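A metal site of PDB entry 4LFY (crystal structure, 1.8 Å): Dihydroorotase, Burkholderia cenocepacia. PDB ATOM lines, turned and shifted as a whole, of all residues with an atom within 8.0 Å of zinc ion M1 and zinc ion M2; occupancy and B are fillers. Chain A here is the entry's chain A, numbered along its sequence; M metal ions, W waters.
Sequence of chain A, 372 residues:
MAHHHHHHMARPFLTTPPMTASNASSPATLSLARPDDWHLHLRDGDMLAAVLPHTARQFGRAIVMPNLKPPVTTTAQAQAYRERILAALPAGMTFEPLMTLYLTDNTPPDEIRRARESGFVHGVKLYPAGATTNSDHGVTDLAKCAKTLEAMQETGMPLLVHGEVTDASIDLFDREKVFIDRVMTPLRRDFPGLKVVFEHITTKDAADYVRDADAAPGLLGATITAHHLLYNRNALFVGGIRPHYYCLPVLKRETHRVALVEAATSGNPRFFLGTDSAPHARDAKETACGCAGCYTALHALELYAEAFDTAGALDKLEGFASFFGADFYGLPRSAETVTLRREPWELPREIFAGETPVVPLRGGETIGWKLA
NZ of KCX 125 lies within hydrogen-bond range of the side-chain hydroxyl (OH) of Tyr 127.
The side-chain sulfur of Met 65 sits at hydrogen-bond distance from NZ of KCX 125 (3.5 Å).
ND1 of His 41 is in hydrogen-bond range of OD1 of Asn 67.
N of His 41 sits at hydrogen-bond distance from O of Ser 277 (3.2 Å).
OE1 of Glu 199 lies within hydrogen-bond range of ND1 of His 39 (2.7 Å).
The backbone carbonyl oxygen (O) of His 39 is in hydrogen-bond range of the side-chain hydroxyl (OG1) of Thr 275 (3.4 Å).
The side-chain carboxylate of Glu 164 lies within hydrogen-bond range of a ring nitrogen (NE2) of His 162 (2.8 Å).
O of Leu 126 sits at hydrogen-bond distance from N of His 162 (3.0 Å).
Four residues have an atom within 4 Å of zinc ion M1: His 39, His 41, KCX 125 and Asp 276.
The nearest printed residue that does not touch zinc ion M1 is His 200 (4.2 Å).
Four residues have an atom within 4 Å of zinc ion M2: His 39, KCX 125, His 162 and His 200.
Water W1 is bound to zinc ion M1, 2.0 Å away.
OQ1 of KCX 125 binds zinc ion M1 (2.1 Å).
NE2 of His 41 binds zinc ion M1 (2.1 Å).
OD1 of Asp 276 binds zinc ion M1 (2.1 Å).
A ring nitrogen (NE2) of His 39 is bound to zinc ion M1, 2.2 Å away.
Zinc ion M1 has five donor atoms within binding distance.
Zinc ion M2 is bound by OQ2 of KCX 125 (1.8 Å), a ring nitrogen (NE2) of His 200 (2.1 Å), water W1 (2.1 Å) and a ring nitrogen (ND1) of His 162 (2.2 Å).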
ATOM      1  N   HIS A  39      11.201  -3.225  21.645  1.00  0.00           N
ATOM      2  CA  HIS A  39      10.270  -2.810  20.582  1.00  0.00           C
ATOM      3  C   HIS A  39      10.449  -3.662  19.339  1.00  0.00           C
ATOM      4  O   HIS A  39      11.347  -3.397  18.564  1.00  0.00           O
ATOM      5  CB  HIS A  39      10.489  -1.325  20.229  1.00  0.00           C
ATOM      6  CG  HIS A  39       9.523  -0.740  19.239  1.00  0.00           C
ATOM      7  ND1 HIS A  39       8.914   0.492  19.438  1.00  0.00           N
ATOM      8  CD2 HIS A  39       9.014  -1.213  18.067  1.00  0.00           C
ATOM      9  CE1 HIS A  39       8.106   0.747  18.416  1.00  0.00           C
ATOM     10  NE2 HIS A  39       8.182  -0.255  17.561  1.00  0.00           N
ATOM     11  N   LEU A  40       9.610  -4.662  19.153  1.00  0.00           N
ATOM     12  CA  LEU A  40       9.796  -5.647  18.096  1.00  0.00           C
ATOM     13  C   LEU A  40       8.528  -5.952  17.328  1.00  0.00           C
ATOM     14  O   LEU A  40       7.444  -6.059  17.927  1.00  0.00           O
ATOM     15  CB  LEU A  40      10.373  -6.901  18.717  1.00  0.00           C
ATOM     16  CG  LEU A  40      10.589  -8.123  17.793  1.00  0.00           C
ATOM     17  CD1 LEU A  40      11.683  -7.851  16.794  1.00  0.00           C
ATOM     18  CD2 LEU A  40      10.969  -9.331  18.640  1.00  0.00           C
ATOM     19  N   HIS A  41       8.673  -6.090  16.018  1.00  0.00           N
ATOM     20  CA  HIS A  41       7.630  -6.645  15.138  1.00  0.00           C
ATOM     21  C   HIS A  41       7.967  -8.054  14.700  1.00  0.00           C
ATOM     22  O   HIS A  41       8.868  -8.246  13.882  1.00  0.00           O
ATOM     23  CB  HIS A  41       7.450  -5.734  13.931  1.00  0.00           C
ATOM     24  CG  HIS A  41       7.033  -4.342  14.317  1.00  0.00           C
ATOM     25  ND1 HIS A  41       5.711  -4.008  14.535  1.00  0.00           N
ATOM     26  CD2 HIS A  41       7.747  -3.243  14.662  1.00  0.00           C
ATOM     27  CE1 HIS A  41       5.637  -2.732  14.927  1.00  0.00           C
ATOM     28  NE2 HIS A  41       6.856  -2.269  15.025  1.00  0.00           N
ATOM     29  N   ARG A  43       5.549 -10.086  13.320  1.00  0.00           N
ATOM     30  CA  ARG A  43       4.572 -10.471  12.257  1.00  0.00           C
ATOM     31  C   ARG A  43       3.853 -11.792  12.619  1.00  0.00           C
ATOM     32  O   ARG A  43       3.687 -12.103  13.809  1.00  0.00           O
ATOM     33  CB  ARG A  43       5.264 -10.587  10.880  1.00  0.00           C
ATOM     34  CG  ARG A  43       6.192  -9.421  10.552  1.00  0.00           C
ATOM     35  CD  ARG A  43       5.452  -8.096  10.538  1.00  0.00           C
ATOM     36  NE  ARG A  43       6.272  -7.024   9.913  1.00  0.00           N
ATOM     37  CZ  ARG A  43       6.085  -5.730  10.081  1.00  0.00           C
ATOM     38  NH1 ARG A  43       5.109  -5.258  10.838  1.00  0.00           N
ATOM     39  NH2 ARG A  43       6.846  -4.871   9.456  1.00  0.00           N
ATOM     40  N   MET A  65       5.019  -6.046  19.317  1.00  0.00           N
ATOM     41  CA  MET A  65       4.063  -5.001  18.926  1.00  0.00           C
ATOM     42  C   MET A  65       2.788  -5.613  18.305  1.00  0.00           C
ATOM     43  O   MET A  65       2.808  -6.773  17.886  1.00  0.00           O
ATOM     44  CB  MET A  65       4.737  -3.975  18.002  1.00  0.00           C
ATOM     45  CG  MET A  65       5.684  -3.046  18.715  1.00  0.00           C
ATOM     46  SD  MET A  65       4.950  -2.167  20.130  1.00  0.00           S
ATOM     47  CE  MET A  65       6.367  -1.203  20.809  1.00  0.00           C
ATOM     48  N   PRO A  66       1.668  -4.875  18.373  1.00  0.00           N
ATOM     49  CA  PRO A  66       0.361  -5.471  18.086  1.00  0.00           C
ATOM     50  C   PRO A  66      -0.244  -5.177  16.713  1.00  0.00           C
ATOM     51  O   PRO A  66      -1.445  -5.485  16.505  1.00  0.00           O
ATOM     52  CB  PRO A  66      -0.535  -4.780  19.145  1.00  0.00           C
ATOM     53  CG  PRO A  66       0.032  -3.400  19.206  1.00  0.00           C
ATOM     54  CD  PRO A  66       1.509  -3.509  18.931  1.00  0.00           C
ATOM     55  N   ASN A  67       0.562  -4.584  15.828  1.00  0.00           N
ATOM     56  CA  ASN A  67       0.081  -4.139  14.513  1.00  0.00           C
ATOM     57  C   ASN A  67       0.031  -5.249  13.446  1.00  0.00           C
ATOM     58  O   ASN A  67       0.518  -5.066  12.329  1.00  0.00           O
ATOM     59  CB  ASN A  67       0.903  -2.963  14.024  1.00  0.00           C
ATOM     60  CG  ASN A  67       2.328  -3.345  13.697  1.00  0.00           C
ATOM     61  OD1 ASN A  67       2.902  -4.231  14.322  1.00  0.00           O
ATOM     62  ND2 ASN A  67       2.939  -2.621  12.747  1.00  0.00           N
ATOM     63  N   KCX A 125       0.002   0.070  23.018  1.00  0.00           N
ATOM     64  CA  KCX A 125       0.653   0.919  22.014  1.00  0.00           C
ATOM     65  CB  KCX A 125       1.127  -0.003  20.915  1.00  0.00           C
ATOM     66  CG  KCX A 125       1.822   0.673  19.757  1.00  0.00           C
ATOM     67  CD  KCX A 125       3.162   1.325  20.226  1.00  0.00           C
ATOM     68  CE  KCX A 125       4.030   1.851  19.112  1.00  0.00           C
ATOM     69  NZ  KCX A 125       4.415   0.766  18.203  1.00  0.00           N
ATOM     70  C   KCX A 125      -0.290   1.896  21.368  1.00  0.00           C
ATOM     71  O   KCX A 125      -1.357   1.497  20.839  1.00  0.00           O
ATOM     72  CX  KCX A 125       5.161   1.024  17.130  1.00  0.00           C
ATOM     73  OQ1 KCX A 125       5.477   0.137  16.295  1.00  0.00           O
ATOM     74  OQ2 KCX A 125       5.591   2.318  16.943  1.00  0.00           O
ATOM     75  N   LEU A 126       0.142   3.149  21.305  1.00  0.00           N
ATOM     76  CA  LEU A 126      -0.565   4.224  20.611  1.00  0.00           C
ATOM     77  C   LEU A 126       0.143   4.534  19.280  1.00  0.00           C
ATOM     78  O   LEU A 126       1.327   4.932  19.218  1.00  0.00           O
ATOM     79  CB  LEU A 126      -0.557   5.496  21.493  1.00  0.00           C
ATOM     80  CG  LEU A 126      -1.024   6.799  20.766  1.00  0.00           C
ATOM     81  CD1 LEU A 126      -2.434   6.659  20.274  1.00  0.00           C
ATOM     82  CD2 LEU A 126      -0.867   8.011  21.646  1.00  0.00           C
ATOM     83  N   TYR A 127      -0.589   4.306  18.182  1.00  0.00           N
ATOM     84  CA  TYR A 127      -0.093   4.663  16.853  1.00  0.00           C
ATOM     85  C   TYR A 127      -0.821   5.897  16.299  1.00  0.00           C
ATOM     86  O   TYR A 127      -2.000   6.006  16.494  1.00  0.00           O
ATOM     87  CB  TYR A 127      -0.387   3.562  15.854  1.00  0.00           C
ATOM     88  CG  TYR A 127       0.466   2.369  15.931  1.00  0.00           C
ATOM     89  CD1 TYR A 127       1.727   2.338  15.293  1.00  0.00           C
ATOM     90  CD2 TYR A 127       0.017   1.227  16.599  1.00  0.00           C
ATOM     91  CE1 TYR A 127       2.516   1.187  15.374  1.00  0.00           C
ATOM     92  CE2 TYR A 127       0.825   0.096  16.715  1.00  0.00           C
ATOM     93  CZ  TYR A 127       2.047   0.042  16.087  1.00  0.00           C
ATOM     94  OH  TYR A 127       2.796  -1.144  16.231  1.00  0.00           O
ATOM     95  N   PRO A 128      -0.137   6.758  15.548  1.00  0.00           N
ATOM     96  CA  PRO A 128      -0.918   7.802  14.859  1.00  0.00           C
ATOM     97  C   PRO A 128      -2.018   7.200  13.984  1.00  0.00           C
ATOM     98  O   PRO A 128      -1.830   6.144  13.430  1.00  0.00           O
ATOM     99  CB  PRO A 128       0.107   8.501  13.949  1.00  0.00           C
ATOM    100  CG  PRO A 128       1.410   7.772  14.076  1.00  0.00           C
ATOM    101  CD  PRO A 128       1.173   6.510  14.897  1.00  0.00           C
ATOM    102  N   VAL A 161       4.308   4.897  22.938  1.00  0.00           N
ATOM    103  CA  VAL A 161       3.880   5.912  21.972  1.00  0.00           C
ATOM    104  C   VAL A 161       4.768   6.004  20.737  1.00  0.00           C
ATOM    105  O   VAL A 161       5.991   6.250  20.851  1.00  0.00           O
ATOM    106  CB  VAL A 161       3.875   7.256  22.702  1.00  0.00           C
ATOM    107  CG1 VAL A 161       3.587   8.366  21.751  1.00  0.00           C
ATOM    108  CG2 VAL A 161       2.853   7.202  23.848  1.00  0.00           C
ATOM    109  N   HIS A 162       4.135   5.880  19.563  1.00  0.00           N
ATOM    110  CA  HIS A 162       4.776   6.234  18.302  1.00  0.00           C
ATOM    111  C   HIS A 162       4.463   7.697  18.126  1.00  0.00           C
ATOM    112  O   HIS A 162       3.343   8.061  17.721  1.00  0.00           O
ATOM    113  CB  HIS A 162       4.220   5.373  17.146  1.00  0.00           C
ATOM    114  CG  HIS A 162       4.805   5.710  15.806  1.00  0.00           C
ATOM    115  ND1 HIS A 162       5.481   4.819  15.020  1.00  0.00           N
ATOM    116  CD2 HIS A 162       4.856   6.889  15.156  1.00  0.00           C
ATOM    117  CE1 HIS A 162       5.873   5.407  13.916  1.00  0.00           C
ATOM    118  NE2 HIS A 162       5.531   6.672  13.976  1.00  0.00           N
ATOM    119  N   GLY A 163       5.434   8.553  18.491  1.00  0.00           N
ATOM    120  CA  GLY A 163       5.191   9.958  18.691  1.00  0.00           C
ATOM    121  C   GLY A 163       5.426  10.760  17.425  1.00  0.00           C
ATOM    122  O   GLY A 163       6.430  11.472  17.314  1.00  0.00           O
ATOM    123  N   GLU A 164       4.511  10.624  16.480  1.00  0.00           N
ATOM    124  CA  GLU A 164       4.424  11.548  15.314  1.00  0.00           C
ATOM    125  C   GLU A 164       3.009  12.025  15.073  1.00  0.00           C
ATOM    126  O   GLU A 164       2.066  11.186  15.125  1.00  0.00           O
ATOM    127  CB  GLU A 164       4.898  10.837  14.065  1.00  0.00           C
ATOM    128  CG  GLU A 164       6.354  10.477  14.064  1.00  0.00           C
ATOM    129  CD  GLU A 164       6.801   9.873  12.767  1.00  0.00           C
ATOM    130  OE1 GLU A 164       6.375   8.774  12.399  1.00  0.00           O
ATOM    131  OE2 GLU A 164       7.540  10.563  12.070  1.00  0.00           O
ATOM    132  N   GLU A 199       8.635   5.753  22.011  1.00  0.00           N
ATOM    133  CA  GLU A 199       9.294   4.725  21.206  1.00  0.00           C
ATOM    134  C   GLU A 199      10.177   5.316  20.153  1.00  0.00           C
ATOM    135  O   GLU A 199       9.869   6.393  19.627  1.00  0.00           O
ATOM    136  CB  GLU A 199       8.326   3.783  20.561  1.00  0.00           C
ATOM    137  CG  GLU A 199       7.492   3.023  21.567  1.00  0.00           C
ATOM    138  CD  GLU A 199       8.292   1.998  22.405  1.00  0.00           C
ATOM    139  OE1 GLU A 199       9.336   1.537  21.928  1.00  0.00           O
ATOM    140  OE2 GLU A 199       7.803   1.634  23.503  1.00  0.00           O
ATOM    141  N   HIS A 200      11.197   4.542  19.802  1.00  0.00           N
ATOM    142  CA  HIS A 200      12.156   4.829  18.722  1.00  0.00           C
ATOM    143  C   HIS A 200      12.300   6.334  18.492  1.00  0.00           C
ATOM    144  O   HIS A 200      11.901   6.855  17.435  1.00  0.00           O
ATOM    145  CB  HIS A 200      11.758   4.130  17.432  1.00  0.00           C
ATOM    146  CG  HIS A 200      10.305   4.219  17.068  1.00  0.00           C
ATOM    147  ND1 HIS A 200       9.597   5.403  17.022  1.00  0.00           N
ATOM    148  CD2 HIS A 200       9.446   3.270  16.637  1.00  0.00           C
ATOM    149  CE1 HIS A 200       8.342   5.166  16.677  1.00  0.00           C
ATOM    150  NE2 HIS A 200       8.227   3.872  16.421  1.00  0.00           N
ATOM    151  N   THR A 225      16.600   2.655  18.264  1.00  0.00           N
ATOM    152  CA  THR A 225      16.911   1.566  17.305  1.00  0.00           C
ATOM    153  C   THR A 225      18.403   1.580  16.952  1.00  0.00           C
ATOM    154  O   THR A 225      19.098   2.556  17.208  1.00  0.00           O
ATOM    155  CB  THR A 225      16.115   1.725  15.999  1.00  0.00           C
ATOM    156  OG1 THR A 225      16.657   2.825  15.285  1.00  0.00           O
ATOM    157  CG2 THR A 225      14.604   1.986  16.266  1.00  0.00           C
ATOM    158  N   LEU A 248       9.627   4.193   9.631  1.00  0.00           N
ATOM    159  CA  LEU A 248       9.037   5.309  10.418  1.00  0.00           C
ATOM    160  C   LEU A 248       9.452   5.114  11.911  1.00  0.00           C
ATOM    161  O   LEU A 248       9.521   4.005  12.419  1.00  0.00           O
ATOM    162  CB  LEU A 248       7.525   5.359  10.276  1.00  0.00           C
ATOM    163  CG  LEU A 248       7.056   5.580   8.829  1.00  0.00           C
ATOM    164  CD1 LEU A 248       5.545   5.509   8.847  1.00  0.00           C
ATOM    165  CD2 LEU A 248       7.496   6.862   8.163  1.00  0.00           C
ATOM    166  N   PRO A 249       9.861   6.173  12.570  1.00  0.00           N
ATOM    167  CA  PRO A 249      10.058   7.478  11.987  1.00  0.00           C
ATOM    168  C   PRO A 249      11.277   7.502  11.073  1.00  0.00           C
ATOM    169  O   PRO A 249      12.236   6.734  11.235  1.00  0.00           O
ATOM    170  CB  PRO A 249      10.225   8.391  13.216  1.00  0.00           C
ATOM    171  CG  PRO A 249       9.981   7.560  14.413  1.00  0.00           C
ATOM    172  CD  PRO A 249      10.273   6.161  13.981  1.00  0.00           C
ATOM    173  N   THR A 275      14.658  -2.478  18.921  1.00  0.00           N
ATOM    174  CA  THR A 275      15.148  -2.528  17.542  1.00  0.00           C
ATOM    175  C   THR A 275      14.213  -1.878  16.544  1.00  0.00           C
ATOM    176  O   THR A 275      14.650  -1.377  15.523  1.00  0.00           O
ATOM    177  CB  THR A 275      15.364  -3.966  17.024  1.00  0.00           C
ATOM    178  OG1 THR A 275      14.130  -4.711  17.091  1.00  0.00           O
ATOM    179  CG2 THR A 275      16.428  -4.659  17.823  1.00  0.00           C
ATOM    180  N   ASP A 276      12.912  -1.948  16.820  1.00  0.00           N
ATOM    181  CA  ASP A 276      11.905  -1.729  15.825  1.00  0.00           C
ATOM    182  C   ASP A 276      12.189  -2.560  14.544  1.00  0.00           C
ATOM    183  O   ASP A 276      11.872  -2.113  13.432  1.00  0.00           O
ATOM    184  CB  ASP A 276      11.734  -0.232  15.472  1.00  0.00           C
ATOM    185  CG  ASP A 276      10.393   0.058  14.810  1.00  0.00           C
ATOM    186  OD1 ASP A 276       9.420  -0.675  15.025  1.00  0.00           O
ATOM    187  OD2 ASP A 276      10.342   1.062  14.082  1.00  0.00           O
ATOM    188  N   SER A 277      12.740  -3.743  14.691  1.00  0.00           N
ATOM    189  CA  SER A 277      12.957  -4.636  13.571  1.00  0.00           C
ATOM    190  C   SER A 277      11.543  -4.943  12.991  1.00  0.00           C
ATOM    191  O   SER A 277      10.663  -5.309  13.697  1.00  0.00           O
ATOM    192  CB  SER A 277      13.616  -5.947  14.007  1.00  0.00           C
ATOM    193  OG  SER A 277      13.736  -6.821  12.858  1.00  0.00           O
ATOM    194  N   ALA A 278      11.378  -4.756  11.680  1.00  0.00           N
ATOM    195  CA  ALA A 278      10.069  -4.581  11.046  1.00  0.00           C
ATOM    196  C   ALA A 278      10.130  -5.166   9.629  1.00  0.00           C
ATOM    197  O   ALA A 278      10.246  -4.415   8.640  1.00  0.00           O
ATOM    198  CB  ALA A 278       9.679  -3.115  11.037  1.00  0.00           C
HETATM  199 ZN    ZN M   1       7.392  -0.288  15.561  1.00  0.00          ZN
HETATM  200 ZN    ZN M   2       6.581   3.008  15.553  1.00  0.00          ZN
HETATM  201  O   HOH W   1       7.399   1.412  14.543  1.00  0.00           O
